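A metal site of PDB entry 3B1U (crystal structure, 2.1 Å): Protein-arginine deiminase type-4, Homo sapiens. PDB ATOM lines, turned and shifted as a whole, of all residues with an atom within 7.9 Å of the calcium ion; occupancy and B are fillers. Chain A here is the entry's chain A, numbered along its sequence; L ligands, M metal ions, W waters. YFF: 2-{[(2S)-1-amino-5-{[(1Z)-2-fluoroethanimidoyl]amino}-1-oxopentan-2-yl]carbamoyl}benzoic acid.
OD1 of Asp 481 is in salt-bridge range of NAC of the ligand (3.8 Å).
OD1 of Asp 358 lies within salt-bridge range of NAC of the ligand, at 2.9 Å.
The calcium ion is bound by the backbone carbonyl oxygen (O) of Phe 415 (2.2 Å), the side-chain amide oxygen (OE1) of Gln 357 (2.3 Å), water W2 (2.3 Å), the side-chain carboxylate (OE1) of Glu 361 (2.4 Å), the backbone carbonyl oxygen (O) of Leu 418 (2.5 Å), water W1 (2.6 Å) and the side-chain carboxylate (OE1) of Glu 419 (2.6 Å).
Five residues have an atom within 4 Å of the calcium ion: Gln 357, Glu 361, Phe 415, Leu 418 and Glu 419.
Water W2 bridges the side-chain carboxylate of Glu 361 (2.7 Å) and the side-chain carboxylate of Glu 419 (3.4 Å).
Water W1 lies within hydrogen-bond range of the backbone carbonyl oxygen of Gln 357 (2.6 Å), the backbone carbonyl oxygen of Met 360 (2.8 Å) and the side-chain amide nitrogen of Asn 656 (3.3 Å).
The side-chain amide nitrogen (NE2) of Gln 357 lies close to the backbone carbonyl oxygen (O) of His 652 (3.3 Å).
The backbone NH (N) of Phe 415 sits at hydrogen-bond distance from the backbone carbonyl oxygen (O) of Asp 358 (2.9 Å).
The backbone NH (N) of Leu 437 is in hydrogen-bond range of the backbone carbonyl oxygen (O) of Glu 419 (2.8 Å).
O of Thr 655 is in hydrogen-bond range of NE2 of Gln 357 (3.0 Å).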
ATOM      1  N   MET A 306     -19.171  -0.577  39.248  1.00  0.00           N
ATOM      2  CA  MET A 306     -19.080  -1.053  37.859  1.00  0.00           C
ATOM      3  C   MET A 306     -20.162  -2.074  37.537  1.00  0.00           C
ATOM      4  O   MET A 306     -20.773  -2.641  38.437  1.00  0.00           O
ATOM      5  CB  MET A 306     -17.714  -1.692  37.602  1.00  0.00           C
ATOM      6  CG  MET A 306     -16.580  -0.712  37.617  1.00  0.00           C
ATOM      7  SD  MET A 306     -14.977  -1.467  37.300  1.00  0.00           S
ATOM      8  CE  MET A 306     -15.239  -2.198  35.704  1.00  0.00           C
ATOM      9  N   THR A 307     -20.371  -2.302  36.237  1.00  0.00           N
ATOM     10  CA  THR A 307     -21.367  -3.258  35.751  1.00  0.00           C
ATOM     11  C   THR A 307     -20.714  -4.311  34.839  1.00  0.00           C
ATOM     12  O   THR A 307     -20.122  -3.958  33.819  1.00  0.00           O
ATOM     13  CB  THR A 307     -22.464  -2.549  34.945  1.00  0.00           C
ATOM     14  OG1 THR A 307     -21.867  -1.777  33.900  1.00  0.00           O
ATOM     15  CG2 THR A 307     -23.283  -1.632  35.853  1.00  0.00           C
ATOM     16  N   ASN A 309     -20.416  -7.771  32.257  1.00  0.00           N
ATOM     17  CA  ASN A 309     -20.989  -8.073  30.944  1.00  0.00           C
ATOM     18  C   ASN A 309     -22.348  -8.769  31.013  1.00  0.00           C
ATOM     19  O   ASN A 309     -23.091  -8.749  30.033  1.00  0.00           O
ATOM     20  CB  ASN A 309     -20.022  -8.951  30.139  1.00  0.00           C
ATOM     21  CG  ASN A 309     -18.752  -8.218  29.736  1.00  0.00           C
ATOM     22  OD1 ASN A 309     -18.639  -7.007  29.889  1.00  0.00           O
ATOM     23  ND2 ASN A 309     -17.782  -8.961  29.211  1.00  0.00           N
ATOM     24  N   MET A 356     -11.738   2.919  22.362  1.00  0.00           N
ATOM     25  CA  MET A 356     -12.833   3.427  23.187  1.00  0.00           C
ATOM     26  C   MET A 356     -12.957   2.701  24.527  1.00  0.00           C
ATOM     27  O   MET A 356     -13.504   3.236  25.487  1.00  0.00           O
ATOM     28  CB  MET A 356     -14.150   3.318  22.403  1.00  0.00           C
ATOM     29  CG  MET A 356     -15.374   3.946  23.067  1.00  0.00           C
ATOM     30  SD  MET A 356     -15.177   5.699  23.456  1.00  0.00           S
ATOM     31  CE  MET A 356     -15.387   6.448  21.844  1.00  0.00           C
ATOM     32  N   GLN A 357     -12.426   1.471  24.585  1.00  0.00           N
ATOM     33  CA  GLN A 357     -12.386   0.689  25.821  1.00  0.00           C
ATOM     34  C   GLN A 357     -11.486   1.318  26.884  1.00  0.00           C
ATOM     35  O   GLN A 357     -11.750   1.207  28.080  1.00  0.00           O
ATOM     36  CB  GLN A 357     -11.879  -0.721  25.512  1.00  0.00           C
ATOM     37  CG  GLN A 357     -11.700  -1.650  26.723  1.00  0.00           C
ATOM     38  CD  GLN A 357     -12.997  -1.960  27.442  1.00  0.00           C
ATOM     39  OE1 GLN A 357     -12.988  -2.281  28.633  1.00  0.00           O
ATOM     40  NE2 GLN A 357     -14.118  -1.893  26.729  1.00  0.00           N
ATOM     41  N   ASP A 358     -10.424   1.966  26.436  1.00  0.00           N
ATOM     42  CA  ASP A 358      -9.278   2.239  27.308  1.00  0.00           C
ATOM     43  C   ASP A 358      -9.339   3.560  28.079  1.00  0.00           C
ATOM     44  O   ASP A 358      -8.800   3.638  29.182  1.00  0.00           O
ATOM     45  CB  ASP A 358      -7.992   2.158  26.481  1.00  0.00           C
ATOM     46  CG  ASP A 358      -7.700   0.747  25.995  1.00  0.00           C
ATOM     47  OD1 ASP A 358      -8.214  -0.229  26.602  1.00  0.00           O
ATOM     48  OD2 ASP A 358      -6.956   0.611  25.014  1.00  0.00           O
ATOM     49  N   MET A 360     -12.038   5.173  29.287  1.00  0.00           N
ATOM     50  CA  MET A 360     -13.087   5.290  30.287  1.00  0.00           C
ATOM     51  C   MET A 360     -13.737   3.968  30.694  1.00  0.00           C
ATOM     52  O   MET A 360     -13.632   2.949  29.990  1.00  0.00           O
ATOM     53  CB  MET A 360     -14.180   6.232  29.791  1.00  0.00           C
ATOM     54  CG  MET A 360     -15.043   5.655  28.676  1.00  0.00           C
ATOM     55  SD  MET A 360     -16.166   6.869  27.962  1.00  0.00           S
ATOM     56  CE  MET A 360     -17.092   5.824  26.851  1.00  0.00           C
ATOM     57  N   GLU A 361     -14.392   3.997  31.854  1.00  0.00           N
ATOM     58  CA  GLU A 361     -15.215   2.895  32.352  1.00  0.00           C
ATOM     59  C   GLU A 361     -16.532   3.496  32.835  1.00  0.00           C
ATOM     60  O   GLU A 361     -16.518   4.442  33.621  1.00  0.00           O
ATOM     61  CB  GLU A 361     -14.503   2.167  33.491  1.00  0.00           C
ATOM     62  CG  GLU A 361     -15.197   0.897  33.984  1.00  0.00           C
ATOM     63  CD  GLU A 361     -15.089  -0.272  33.007  1.00  0.00           C
ATOM     64  OE1 GLU A 361     -13.993  -0.489  32.446  1.00  0.00           O
ATOM     65  OE2 GLU A 361     -16.099  -0.988  32.819  1.00  0.00           O
ATOM     66  N   ILE A 362     -17.642   2.957  32.353  1.00  0.00           N
ATOM     67  CA  ILE A 362     -18.953   3.493  32.701  1.00  0.00           C
ATOM     68  C   ILE A 362     -19.557   2.687  33.851  1.00  0.00           C
ATOM     69  O   ILE A 362     -19.915   1.524  33.673  1.00  0.00           O
ATOM     70  CB  ILE A 362     -19.930   3.486  31.496  1.00  0.00           C
ATOM     71  CG1 ILE A 362     -19.257   4.064  30.246  1.00  0.00           C
ATOM     72  CG2 ILE A 362     -21.197   4.272  31.833  1.00  0.00           C
ATOM     73  CD1 ILE A 362     -18.712   5.463  30.415  1.00  0.00           C
ATOM     74  N   SER A 414      -4.905   1.822  31.325  1.00  0.00           N
ATOM     75  CA  SER A 414      -5.972   1.775  30.326  1.00  0.00           C
ATOM     76  C   SER A 414      -7.057   0.821  30.804  1.00  0.00           C
ATOM     77  O   SER A 414      -6.754  -0.256  31.308  1.00  0.00           O
ATOM     78  CB  SER A 414      -5.429   1.309  28.981  1.00  0.00           C
ATOM     79  OG  SER A 414      -4.508   2.244  28.438  1.00  0.00           O
ATOM     80  N   PHE A 415      -8.316   1.213  30.652  1.00  0.00           N
ATOM     81  CA  PHE A 415      -9.420   0.504  31.308  1.00  0.00           C
ATOM     82  C   PHE A 415      -9.937  -0.740  30.580  1.00  0.00           C
ATOM     83  O   PHE A 415     -10.955  -1.314  30.972  1.00  0.00           O
ATOM     84  CB  PHE A 415     -10.556   1.474  31.666  1.00  0.00           C
ATOM     85  CG  PHE A 415     -10.233   2.411  32.820  1.00  0.00           C
ATOM     86  CD1 PHE A 415     -11.110   3.426  33.170  1.00  0.00           C
ATOM     87  CD2 PHE A 415      -9.042   2.288  33.552  1.00  0.00           C
ATOM     88  CE1 PHE A 415     -10.842   4.283  34.223  1.00  0.00           C
ATOM     89  CE2 PHE A 415      -8.762   3.152  34.610  1.00  0.00           C
ATOM     90  CZ  PHE A 415      -9.663   4.146  34.939  1.00  0.00           C
ATOM     91  N   GLY A 416      -9.209  -1.177  29.548  1.00  0.00           N
ATOM     92  CA  GLY A 416      -9.303  -2.565  29.095  1.00  0.00           C
ATOM     93  C   GLY A 416      -8.742  -3.490  30.165  1.00  0.00           C
ATOM     94  O   GLY A 416      -9.056  -4.677  30.206  1.00  0.00           O
ATOM     95  N   ASN A 417      -7.906  -2.916  31.036  1.00  0.00           N
ATOM     96  CA  ASN A 417      -7.361  -3.612  32.203  1.00  0.00           C
ATOM     97  C   ASN A 417      -8.245  -3.484  33.455  1.00  0.00           C
ATOM     98  O   ASN A 417      -7.799  -3.796  34.564  1.00  0.00           O
ATOM     99  CB  ASN A 417      -5.958  -3.082  32.497  1.00  0.00           C
ATOM    100  CG  ASN A 417      -5.166  -3.984  33.428  1.00  0.00           C
ATOM    101  OD1 ASN A 417      -5.241  -5.212  33.346  1.00  0.00           O
ATOM    102  ND2 ASN A 417      -4.415  -3.377  34.340  1.00  0.00           N
ATOM    103  N   LEU A 418      -9.476  -3.013  33.285  1.00  0.00           N
ATOM    104  CA  LEU A 418     -10.411  -2.851  34.402  1.00  0.00           C
ATOM    105  C   LEU A 418     -11.758  -3.484  34.048  1.00  0.00           C
ATOM    106  O   LEU A 418     -12.440  -3.028  33.128  1.00  0.00           O
ATOM    107  CB  LEU A 418     -10.589  -1.360  34.715  1.00  0.00           C
ATOM    108  CG  LEU A 418     -11.478  -0.988  35.905  1.00  0.00           C
ATOM    109  CD1 LEU A 418     -11.033  -1.670  37.188  1.00  0.00           C
ATOM    110  CD2 LEU A 418     -11.512   0.525  36.083  1.00  0.00           C
ATOM    111  N   GLU A 419     -12.116  -4.543  34.771  1.00  0.00           N
ATOM    112  CA  GLU A 419     -13.325  -5.313  34.507  1.00  0.00           C
ATOM    113  C   GLU A 419     -13.997  -5.689  35.828  1.00  0.00           C
ATOM    114  O   GLU A 419     -13.473  -5.391  36.914  1.00  0.00           O
ATOM    115  CB  GLU A 419     -12.989  -6.581  33.716  1.00  0.00           C
ATOM    116  CG  GLU A 419     -12.281  -6.338  32.375  1.00  0.00           C
ATOM    117  CD  GLU A 419     -13.161  -5.623  31.352  1.00  0.00           C
ATOM    118  OE1 GLU A 419     -12.677  -4.667  30.717  1.00  0.00           O
ATOM    119  OE2 GLU A 419     -14.335  -6.003  31.204  1.00  0.00           O
ATOM    120  N   VAL A 420     -15.166  -6.340  35.740  1.00  0.00           N
ATOM    121  CA  VAL A 420     -15.883  -6.838  36.926  1.00  0.00           C
ATOM    122  C   VAL A 420     -16.503  -8.181  36.627  1.00  0.00           C
ATOM    123  O   VAL A 420     -16.993  -8.415  35.531  1.00  0.00           O
ATOM    124  CB  VAL A 420     -17.080  -5.935  37.329  1.00  0.00           C
ATOM    125  CG1 VAL A 420     -17.054  -5.646  38.810  1.00  0.00           C
ATOM    126  CG2 VAL A 420     -17.109  -4.663  36.508  1.00  0.00           C
ATOM    127  N   LEU A 437     -11.952  -6.756  38.767  1.00  0.00           N
ATOM    128  CA  LEU A 437     -10.770  -7.473  38.334  1.00  0.00           C
ATOM    129  C   LEU A 437      -9.874  -6.480  37.611  1.00  0.00           C
ATOM    130  O   LEU A 437     -10.344  -5.748  36.741  1.00  0.00           O
ATOM    131  CB  LEU A 437     -11.166  -8.582  37.342  1.00  0.00           C
ATOM    132  CG  LEU A 437     -11.722  -9.934  37.801  1.00  0.00           C
ATOM    133  CD1 LEU A 437     -12.256  -9.945  39.209  1.00  0.00           C
ATOM    134  CD2 LEU A 437     -12.778 -10.426  36.800  1.00  0.00           C
ATOM    135  N   VAL A 480      -6.465  -7.386  31.243  1.00  0.00           N
ATOM    136  CA  VAL A 480      -7.229  -8.593  31.578  1.00  0.00           C
ATOM    137  C   VAL A 480      -8.249  -8.989  30.503  1.00  0.00           C
ATOM    138  O   VAL A 480      -8.547 -10.167  30.355  1.00  0.00           O
ATOM    139  CB  VAL A 480      -7.946  -8.476  32.942  1.00  0.00           C
ATOM    140  CG1 VAL A 480      -6.937  -8.430  34.086  1.00  0.00           C
ATOM    141  CG2 VAL A 480      -8.878  -7.262  32.977  1.00  0.00           C
ATOM    142  N   ASP A 481      -8.758  -8.015  29.748  1.00  0.00           N
ATOM    143  CA  ASP A 481      -9.709  -8.303  28.663  1.00  0.00           C
ATOM    144  C   ASP A 481      -9.065  -9.038  27.469  1.00  0.00           C
ATOM    145  O   ASP A 481      -9.764  -9.540  26.597  1.00  0.00           O
ATOM    146  CB  ASP A 481     -10.447  -7.028  28.199  1.00  0.00           C
ATOM    147  CG  ASP A 481      -9.578  -6.099  27.342  1.00  0.00           C
ATOM    148  OD1 ASP A 481     -10.171  -5.262  26.621  1.00  0.00           O
ATOM    149  OD2 ASP A 481      -8.339  -6.195  27.383  1.00  0.00           O
ATOM    150  N   HIS A 652     -13.560  -5.653  21.525  1.00  0.00           N
ATOM    151  CA  HIS A 652     -13.773  -5.141  22.883  1.00  0.00           C
ATOM    152  C   HIS A 652     -12.923  -3.892  23.128  1.00  0.00           C
ATOM    153  O   HIS A 652     -13.403  -2.927  23.713  1.00  0.00           O
ATOM    154  CB  HIS A 652     -13.448  -6.210  23.939  1.00  0.00           C
ATOM    155  CG  HIS A 652     -13.884  -5.857  25.323  1.00  0.00           C
ATOM    156  ND1 HIS A 652     -12.996  -5.408  26.288  1.00  0.00           N
ATOM    157  CD2 HIS A 652     -15.096  -5.885  25.926  1.00  0.00           C
ATOM    158  CE1 HIS A 652     -13.654  -5.179  27.409  1.00  0.00           C
ATOM    159  NE2 HIS A 652     -14.930  -5.465  27.216  1.00  0.00           N
ATOM    160  N   THR A 655     -14.357  -0.684  21.525  1.00  0.00           N
ATOM    161  CA  THR A 655     -15.715  -0.307  21.940  1.00  0.00           C
ATOM    162  C   THR A 655     -15.854  -0.205  23.452  1.00  0.00           C
ATOM    163  O   THR A 655     -14.937  -0.531  24.210  1.00  0.00           O
ATOM    164  CB  THR A 655     -16.763  -1.318  21.429  1.00  0.00           C
ATOM    165  OG1 THR A 655     -16.545  -2.599  22.041  1.00  0.00           O
ATOM    166  CG2 THR A 655     -16.694  -1.469  19.905  1.00  0.00           C
ATOM    167  N   ASN A 656     -17.016   0.279  23.886  1.00  0.00           N
ATOM    168  CA  ASN A 656     -17.354   0.333  25.309  1.00  0.00           C
ATOM    169  C   ASN A 656     -18.873   0.296  25.465  1.00  0.00           C
ATOM    170  O   ASN A 656     -19.601   0.591  24.510  1.00  0.00           O
ATOM    171  CB  ASN A 656     -16.772   1.603  25.949  1.00  0.00           C
ATOM    172  CG  ASN A 656     -16.373   1.394  27.387  1.00  0.00           C
ATOM    173  OD1 ASN A 656     -17.069   0.720  28.147  1.00  0.00           O
ATOM    174  ND2 ASN A 656     -15.249   1.973  27.785  1.00  0.00           N
ATOM    175  N   VAL A 657     -19.337  -0.078  26.651  1.00  0.00           N
ATOM    176  CA  VAL A 657     -20.782  -0.253  26.884  1.00  0.00           C
ATOM    177  C   VAL A 657     -21.221   0.314  28.230  1.00  0.00           C
ATOM    178  O   VAL A 657     -20.550   0.122  29.245  1.00  0.00           O
ATOM    179  CB  VAL A 657     -21.177  -1.747  26.822  1.00  0.00           C
ATOM    180  CG1 VAL A 657     -22.683  -1.904  26.976  1.00  0.00           C
ATOM    181  CG2 VAL A 657     -20.694  -2.387  25.528  1.00  0.00           C
ATOM    182  N   ARG A 659     -24.186  -0.165  30.904  1.00  0.00           N
ATOM    183  CA  ARG A 659     -25.114  -1.246  31.244  1.00  0.00           C
ATOM    184  C   ARG A 659     -26.008  -0.880  32.414  1.00  0.00           C
ATOM    185  O   ARG A 659     -25.712   0.048  33.184  1.00  0.00           O
ATOM    186  CB  ARG A 659     -24.323  -2.514  31.568  1.00  0.00           C
ATOM    187  CG  ARG A 659     -23.326  -2.891  30.496  1.00  0.00           C
ATOM    188  CD  ARG A 659     -22.653  -4.215  30.781  1.00  0.00           C
ATOM    189  NE  ARG A 659     -22.179  -4.829  29.546  1.00  0.00           N
ATOM    190  CZ  ARG A 659     -20.977  -4.664  29.008  1.00  0.00           C
ATOM    191  NH1 ARG A 659     -20.050  -3.904  29.589  1.00  0.00           N
ATOM    192  NH2 ARG A 659     -20.691  -5.291  27.865  1.00  0.00           N
HETATM  193  C1  YFF L   1      -2.164   3.270  17.985  1.00  0.00           C
HETATM  194  O1  YFF L   1      -1.691   4.420  17.871  1.00  0.00           O
HETATM  195  O2  YFF L   1      -3.370   3.081  18.273  1.00  0.00           O
HETATM  196  NAA YFF L   1      -1.055  -0.447  22.946  1.00  0.00           N
HETATM  197  NAC YFF L   1      -7.691  -2.752  25.313  1.00  0.00           N
HETATM  198  OAE YFF L   1      -2.570   0.878  23.914  1.00  0.00           O
HETATM  199  OAF YFF L   1      -1.505   2.182  20.790  1.00  0.00           O
HETATM  200  CAH YFF L   1       0.200   0.886  16.245  1.00  0.00           C
HETATM  201  CAI YFF L   1      -0.646   1.970  16.512  1.00  0.00           C
HETATM  202  CAJ YFF L   1       0.417  -0.073  17.225  1.00  0.00           C
HETATM  203  CAK YFF L   1      -1.270   2.086  17.753  1.00  0.00           C
HETATM  204  CAL YFF L   1      -0.201   0.051  18.462  1.00  0.00           C
HETATM  205  CAM YFF L   1      -4.106  -1.935  23.096  1.00  0.00           C
HETATM  206  CAN YFF L   1      -5.548  -1.702  23.533  1.00  0.00           C
HETATM  207  CAO YFF L   1      -3.768  -1.348  21.725  1.00  0.00           C
HETATM  208  CAP YFF L   1      -7.493  -4.935  24.249  1.00  0.00           C
HETATM  209  NAR YFF L   1      -6.125  -3.035  23.593  1.00  0.00           N
HETATM  210  NAS YFF L   1      -2.429   0.150  20.481  1.00  0.00           N
HETATM  211  CAU YFF L   1      -2.212   0.192  22.966  1.00  0.00           C
HETATM  212  CAV YFF L   1      -7.083  -3.501  24.397  1.00  0.00           C
HETATM  213  CAW YFF L   1      -1.688   1.195  20.094  1.00  0.00           C
HETATM  214  CAX YFF L   1      -1.053   1.127  18.732  1.00  0.00           C
HETATM  215  CAZ YFF L   1      -3.124   0.044  21.768  1.00  0.00           C
HETATM  216 CA    CA M   1     -13.051  -2.097  30.935  1.00  0.00          CA
HETATM  217  O   HOH W   1     -13.400   0.166  29.759  1.00  0.00           O
HETATM  218  O   HOH W   2     -15.315  -2.713  30.921  1.00  0.00           O
